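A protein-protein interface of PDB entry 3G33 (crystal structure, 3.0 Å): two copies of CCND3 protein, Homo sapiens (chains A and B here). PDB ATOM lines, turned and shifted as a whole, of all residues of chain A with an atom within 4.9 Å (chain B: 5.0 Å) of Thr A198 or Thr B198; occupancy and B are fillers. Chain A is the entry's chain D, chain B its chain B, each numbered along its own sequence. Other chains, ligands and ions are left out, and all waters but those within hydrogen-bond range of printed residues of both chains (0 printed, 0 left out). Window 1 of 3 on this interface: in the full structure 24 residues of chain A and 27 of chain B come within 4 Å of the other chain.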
ATOM      1  N   LEU A 191      23.034   6.660   9.922  1.00  0.00           N
ATOM      2  CA  LEU A 191      22.063   5.805   9.241  1.00  0.00           C
ATOM      3  C   LEU A 191      22.296   5.714   7.736  1.00  0.00           C
ATOM      4  O   LEU A 191      22.226   4.631   7.156  1.00  0.00           O
ATOM      5  CB  LEU A 191      20.633   6.270   9.521  1.00  0.00           C
ATOM      6  CG  LEU A 191      19.896   5.517  10.628  1.00  0.00           C
ATOM      7  CD1 LEU A 191      18.517   6.113  10.858  1.00  0.00           C
ATOM      8  CD2 LEU A 191      19.794   4.039  10.278  1.00  0.00           C
ATOM      9  N   LYS A 194      25.253   3.406   6.937  1.00  0.00           N
ATOM     10  CA  LYS A 194      24.958   1.996   7.158  1.00  0.00           C
ATOM     11  C   LYS A 194      24.112   1.428   6.024  1.00  0.00           C
ATOM     12  O   LYS A 194      24.436   0.386   5.453  1.00  0.00           O
ATOM     13  CB  LYS A 194      24.248   1.787   8.496  1.00  0.00           C
ATOM     14  CG  LYS A 194      24.087   0.323   8.862  1.00  0.00           C
ATOM     15  CD  LYS A 194      23.395   0.136  10.203  1.00  0.00           C
ATOM     16  CE  LYS A 194      23.467  -1.319  10.635  1.00  0.00           C
ATOM     17  NZ  LYS A 194      22.544  -1.615  11.758  1.00  0.00           N
ATOM     18  N   HIS A 195      23.027   2.124   5.703  1.00  0.00           N
ATOM     19  CA  HIS A 195      22.124   1.692   4.645  1.00  0.00           C
ATOM     20  C   HIS A 195      22.853   1.578   3.311  1.00  0.00           C
ATOM     21  O   HIS A 195      22.592   0.667   2.525  1.00  0.00           O
ATOM     22  CB  HIS A 195      20.944   2.658   4.528  1.00  0.00           C
ATOM     23  CG  HIS A 195      19.889   2.213   3.565  1.00  0.00           C
ATOM     24  ND1 HIS A 195      19.367   0.938   3.572  1.00  0.00           N
ATOM     25  CD2 HIS A 195      19.247   2.877   2.576  1.00  0.00           C
ATOM     26  CE1 HIS A 195      18.455   0.832   2.621  1.00  0.00           C
ATOM     27  NE2 HIS A 195      18.363   1.996   2.003  1.00  0.00           N
ATOM     28  N   ALA A 196      23.773   2.503   3.061  1.00  0.00           N
ATOM     29  CA  ALA A 196      24.530   2.504   1.816  1.00  0.00           C
ATOM     30  C   ALA A 196      25.397   1.254   1.689  1.00  0.00           C
ATOM     31  O   ALA A 196      25.693   0.802   0.585  1.00  0.00           O
ATOM     32  CB  ALA A 196      25.386   3.757   1.718  1.00  0.00           C
ATOM     33  N   GLN A 197      25.794   0.695   2.826  1.00  0.00           N
ATOM     34  CA  GLN A 197      26.710  -0.440   2.838  1.00  0.00           C
ATOM     35  C   GLN A 197      26.054  -1.761   2.444  1.00  0.00           C
ATOM     36  O   GLN A 197      26.738  -2.690   2.016  1.00  0.00           O
ATOM     37  CB  GLN A 197      27.392  -0.567   4.202  1.00  0.00           C
ATOM     38  CG  GLN A 197      28.513   0.434   4.415  1.00  0.00           C
ATOM     39  CD  GLN A 197      28.999   0.470   5.847  1.00  0.00           C
ATOM     40  OE1 GLN A 197      28.257   0.145   6.775  1.00  0.00           O
ATOM     41  NE2 GLN A 197      30.252   0.871   6.037  1.00  0.00           N
ATOM     42  N   THR A 198      24.737  -1.852   2.590  1.00  0.00           N
ATOM     43  CA  THR A 198      24.033  -3.059   2.174  1.00  0.00           C
ATOM     44  C   THR A 198      23.930  -3.088   0.654  1.00  0.00           C
ATOM     45  O   THR A 198      23.969  -4.154   0.040  1.00  0.00           O
ATOM     46  CB  THR A 198      22.631  -3.167   2.805  1.00  0.00           C
ATOM     47  OG1 THR A 198      21.697  -2.398   2.040  1.00  0.00           O
ATOM     48  CG2 THR A 198      22.651  -2.671   4.241  1.00  0.00           C
ATOM     49  N   PHE A 199      23.801  -1.910   0.051  1.00  0.00           N
ATOM     50  CA  PHE A 199      23.839  -1.794  -1.401  1.00  0.00           C
ATOM     51  C   PHE A 199      25.231  -2.164  -1.901  1.00  0.00           C
ATOM     52  O   PHE A 199      25.379  -2.828  -2.928  1.00  0.00           O
ATOM     53  CB  PHE A 199      23.482  -0.374  -1.845  1.00  0.00           C
ATOM     54  CG  PHE A 199      22.037  -0.017  -1.638  1.00  0.00           C
ATOM     55  CD1 PHE A 199      21.057  -0.523  -2.476  1.00  0.00           C
ATOM     56  CD2 PHE A 199      21.659   0.836  -0.613  1.00  0.00           C
ATOM     57  CE1 PHE A 199      19.728  -0.194  -2.290  1.00  0.00           C
ATOM     58  CE2 PHE A 199      20.331   1.170  -0.424  1.00  0.00           C
ATOM     59  CZ  PHE A 199      19.365   0.654  -1.263  1.00  0.00           C
ATOM     60  N   LEU A 200      26.248  -1.728  -1.165  1.00  0.00           N
ATOM     61  CA  LEU A 200      27.632  -2.037  -1.502  1.00  0.00           C
ATOM     62  C   LEU A 200      27.887  -3.536  -1.427  1.00  0.00           C
ATOM     63  O   LEU A 200      28.552  -4.106  -2.291  1.00  0.00           O
ATOM     64  CB  LEU A 200      28.592  -1.294  -0.572  1.00  0.00           C
ATOM     65  CG  LEU A 200      28.678   0.223  -0.757  1.00  0.00           C
ATOM     66  CD1 LEU A 200      29.545   0.848   0.324  1.00  0.00           C
ATOM     67  CD2 LEU A 200      29.211   0.565  -2.139  1.00  0.00           C
ATOM     68  N   ALA A 201      27.359  -4.171  -0.387  1.00  0.00           N
ATOM     69  CA  ALA A 201      27.470  -5.615  -0.249  1.00  0.00           C
ATOM     70  C   ALA A 201      26.675  -6.305  -1.351  1.00  0.00           C
ATOM     71  O   ALA A 201      27.094  -7.335  -1.882  1.00  0.00           O
ATOM     72  CB  ALA A 201      26.979  -6.055   1.122  1.00  0.00           C
ATOM     73  N   LEU A 202      25.526  -5.729  -1.690  1.00  0.00           N
ATOM     74  CA  LEU A 202      24.677  -6.270  -2.741  1.00  0.00           C
ATOM     75  C   LEU A 202      25.472  -6.375  -4.034  1.00  0.00           C
ATOM     76  O   LEU A 202      25.532  -7.434  -4.658  1.00  0.00           O
ATOM     77  CB  LEU A 202      23.461  -5.369  -2.957  1.00  0.00           C
ATOM     78  CG  LEU A 202      22.286  -5.971  -3.729  1.00  0.00           C
ATOM     79  CD1 LEU A 202      21.474  -4.873  -4.398  1.00  0.00           C
ATOM     80  CD2 LEU A 202      22.776  -6.972  -4.759  1.00  0.00           C
ATOM     81  N   LEU B 191      21.814 -11.296   3.268  1.00  0.00           N
ATOM     82  CA  LEU B 191      21.401  -9.955   2.857  1.00  0.00           C
ATOM     83  C   LEU B 191      20.149  -9.464   3.579  1.00  0.00           C
ATOM     84  O   LEU B 191      20.085  -8.314   4.011  1.00  0.00           O
ATOM     85  CB  LEU B 191      21.191  -9.889   1.343  1.00  0.00           C
ATOM     86  CG  LEU B 191      22.363  -9.329   0.535  1.00  0.00           C
ATOM     87  CD1 LEU B 191      22.063  -9.378  -0.954  1.00  0.00           C
ATOM     88  CD2 LEU B 191      22.674  -7.906   0.977  1.00  0.00           C
ATOM     89  N   LYS B 194      20.961  -8.368   7.160  1.00  0.00           N
ATOM     90  CA  LYS B 194      21.714  -7.122   7.226  1.00  0.00           C
ATOM     91  C   LYS B 194      20.807  -5.923   6.983  1.00  0.00           C
ATOM     92  O   LYS B 194      20.819  -4.958   7.747  1.00  0.00           O
ATOM     93  CB  LYS B 194      22.863  -7.119   6.218  1.00  0.00           C
ATOM     94  CG  LYS B 194      23.783  -5.921   6.369  1.00  0.00           C
ATOM     95  CD  LYS B 194      24.922  -5.939   5.362  1.00  0.00           C
ATOM     96  CE  LYS B 194      25.945  -4.866   5.700  1.00  0.00           C
ATOM     97  NZ  LYS B 194      26.905  -4.636   4.594  1.00  0.00           N
ATOM     98  N   HIS B 195      20.021  -5.992   5.916  1.00  0.00           N
ATOM     99  CA  HIS B 195      19.114  -4.910   5.564  1.00  0.00           C
ATOM    100  C   HIS B 195      18.115  -4.647   6.685  1.00  0.00           C
ATOM    101  O   HIS B 195      17.768  -3.501   6.965  1.00  0.00           O
ATOM    102  CB  HIS B 195      18.383  -5.238   4.259  1.00  0.00           C
ATOM    103  CG  HIS B 195      17.531  -4.120   3.745  1.00  0.00           C
ATOM    104  ND1 HIS B 195      17.991  -2.824   3.636  1.00  0.00           N
ATOM    105  CD2 HIS B 195      16.254  -4.106   3.296  1.00  0.00           C
ATOM    106  CE1 HIS B 195      17.030  -2.059   3.151  1.00  0.00           C
ATOM    107  NE2 HIS B 195      15.967  -2.812   2.934  1.00  0.00           N
ATOM    108  N   ALA B 196      17.660  -5.716   7.331  1.00  0.00           N
ATOM    109  CA  ALA B 196      16.692  -5.597   8.414  1.00  0.00           C
ATOM    110  C   ALA B 196      17.270  -4.819   9.590  1.00  0.00           C
ATOM    111  O   ALA B 196      16.536  -4.176  10.339  1.00  0.00           O
ATOM    112  CB  ALA B 196      16.233  -6.975   8.863  1.00  0.00           C
ATOM    113  N   GLN B 197      18.588  -4.876   9.742  1.00  0.00           N
ATOM    114  CA  GLN B 197      19.254  -4.266  10.890  1.00  0.00           C
ATOM    115  C   GLN B 197      19.354  -2.745  10.806  1.00  0.00           C
ATOM    116  O   GLN B 197      19.499  -2.074  11.827  1.00  0.00           O
ATOM    117  CB  GLN B 197      20.640  -4.882  11.094  1.00  0.00           C
ATOM    118  CG  GLN B 197      20.602  -6.248  11.758  1.00  0.00           C
ATOM    119  CD  GLN B 197      21.943  -6.948  11.732  1.00  0.00           C
ATOM    120  OE1 GLN B 197      22.770  -6.699  10.854  1.00  0.00           O
ATOM    121  NE2 GLN B 197      22.165  -7.836  12.697  1.00  0.00           N
ATOM    122  N   THR B 198      19.281  -2.199   9.597  1.00  0.00           N
ATOM    123  CA  THR B 198      19.305  -0.751   9.439  1.00  0.00           C
ATOM    124  C   THR B 198      17.953  -0.175   9.844  1.00  0.00           C
ATOM    125  O   THR B 198      17.874   0.929  10.381  1.00  0.00           O
ATOM    126  CB  THR B 198      19.657  -0.323   7.999  1.00  0.00           C
ATOM    127  OG1 THR B 198      18.483  -0.357   7.181  1.00  0.00           O
ATOM    128  CG2 THR B 198      20.719  -1.241   7.412  1.00  0.00           C
ATOM    129  N   PHE B 199      16.891  -0.933   9.587  1.00  0.00           N
ATOM    130  CA  PHE B 199      15.563  -0.558  10.057  1.00  0.00           C
ATOM    131  C   PHE B 199      15.529  -0.614  11.582  1.00  0.00           C
ATOM    132  O   PHE B 199      14.940   0.247  12.235  1.00  0.00           O
ATOM    133  CB  PHE B 199      14.496  -1.487   9.472  1.00  0.00           C
ATOM    134  CG  PHE B 199      14.266  -1.299   8.000  1.00  0.00           C
ATOM    135  CD1 PHE B 199      13.566  -0.199   7.531  1.00  0.00           C
ATOM    136  CD2 PHE B 199      14.737  -2.227   7.085  1.00  0.00           C
ATOM    137  CE1 PHE B 199      13.348  -0.025   6.176  1.00  0.00           C
ATOM    138  CE2 PHE B 199      14.521  -2.058   5.730  1.00  0.00           C
ATOM    139  CZ  PHE B 199      13.826  -0.955   5.276  1.00  0.00           C
ATOM    140  N   LEU B 200      16.171  -1.636  12.141  1.00  0.00           N
ATOM    141  CA  LEU B 200      16.257  -1.795  13.585  1.00  0.00           C
ATOM    142  C   LEU B 200      17.015  -0.634  14.216  1.00  0.00           C
ATOM    143  O   LEU B 200      16.618  -0.115  15.259  1.00  0.00           O
ATOM    144  CB  LEU B 200      16.933  -3.120  13.939  1.00  0.00           C
ATOM    145  CG  LEU B 200      16.136  -4.389  13.638  1.00  0.00           C
ATOM    146  CD1 LEU B 200      16.979  -5.629  13.890  1.00  0.00           C
ATOM    147  CD2 LEU B 200      14.861  -4.430  14.463  1.00  0.00           C
ATOM    148  N   ALA B 201      18.109  -0.230  13.582  1.00  0.00           N
ATOM    149  CA  ALA B 201      18.877   0.914  14.049  1.00  0.00           C
ATOM    150  C   ALA B 201      18.057   2.189  13.882  1.00  0.00           C
ATOM    151  O   ALA B 201      18.103   3.085  14.724  1.00  0.00           O
ATOM    152  CB  ALA B 201      20.191   1.019  13.289  1.00  0.00           C
ATOM    153  N   LEU B 202      17.307   2.258  12.788  1.00  0.00           N
ATOM    154  CA  LEU B 202      16.451   3.402  12.517  1.00  0.00           C
ATOM    155  C   LEU B 202      15.493   3.613  13.679  1.00  0.00           C
ATOM    156  O   LEU B 202      15.402   4.706  14.238  1.00  0.00           O
ATOM    157  CB  LEU B 202      15.658   3.180  11.228  1.00  0.00           C
ATOM    158  CG  LEU B 202      15.015   4.413  10.591  1.00  0.00           C
ATOM    159  CD1 LEU B 202      13.807   4.012   9.759  1.00  0.00           C
ATOM    160  CD2 LEU B 202      14.619   5.429  11.650  1.00  0.00           C
ATOM    161  N   LEU B 265      12.057   6.029   7.520  1.00  0.00           N
ATOM    162  CA  LEU B 265      13.324   5.863   6.820  1.00  0.00           C
ATOM    163  C   LEU B 265      13.523   6.960   5.780  1.00  0.00           C
ATOM    164  O   LEU B 265      14.575   7.599   5.728  1.00  0.00           O
ATOM    165  CB  LEU B 265      13.384   4.492   6.145  1.00  0.00           C
ATOM    166  CG  LEU B 265      14.740   4.068   5.579  1.00  0.00           C
ATOM    167  CD1 LEU B 265      15.712   3.751   6.705  1.00  0.00           C
ATOM    168  CD2 LEU B 265      14.587   2.871   4.654  1.00  0.00           C
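Printed residues of chain B within 4 Å of Leu A191: Thr B198 (3.7 Å) and Leu B202 (3.8 Å).
Printed residues of chain B within 4 Å of Gln A197: Lys B194.
Of chain B, only Thr B198 comes within 4 Å of Thr A198.
Ala B196 touches none of the printed residues of chain A.
Printed residues of chain A within 4 Å of Gln B197: Lys A194 (3.1 Å).
Thr B198 touches just these residues of chain A: Leu A191, Lys A194, His A195 and Thr A198.
Phe B199 touches none of the printed residues of chain A.
Printed residues of chain A within 4 Å of Leu B202: Leu A191 (3.8 Å).
The nearest printed residue of chain A that does not touch Thr B198 is Ala A196 (6.5 Å).
Leu A191 touches Leu B202, but with the chains exchanged Leu A202 does not touch Leu B191 (4.4 Å).
Lys A194 touches Gln B197, and with the chains exchanged Gln A197 touches Lys B194.
His A195 touches its own counterpart, His B195.
Thr A198 touches its own counterpart, Thr B198.
Positions printed for both chains: 191, 194, 195, 196, 197, 198, 199, 200, 201 and 202.
Of the 10 pairs that touch across the chains among the printed residues, 6 have their exchanged pair printed and touching as well.
O of His B195 sits at hydrogen-bond distance from OG1 of Thr B198, at 3.2 Å.
O of His A195 is in hydrogen-bond range of OG1 of Thr A198 (3.2 Å).
Among the printed residues, merely in contact across the chains: Leu A191 with Thr B198, Leu A191 with Leu B202, Lys A194 with Thr B198, Lys A194 with Ala B201, His A195 with His B195, His A195 with Thr B198, Thr A198 with Thr B198 and Ala A201 with Lys B194.
Of the 11 printed residues of chain B, 6 touch a printed residue of chain A.
Hydrophobic or aromatic side chains of chain B within 4 Å of the printed part of chain A: His B195, Ala B201 and Leu B202.
Of the 10 printed residues of chain A, 6 touch a printed residue of chain B.
Hydrophobic or aromatic side chains of chain A within 4 Å of the printed part of chain B: Leu A191, His A195 and Ala A201.
Among the printed residues, no Asp or Glu carboxylate lies within 4 Å of a Lys or Arg side-chain nitrogen of the other chain.
The side-chain amino group (NZ) of Lys B194 lies within hydrogen-bond range of the backbone carbonyl oxygen (O) of Gln A197 (3.2 Å).
The side-chain amino group of Lys A194 is in hydrogen-bond range of the backbone carbonyl oxygen of Gln B197.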
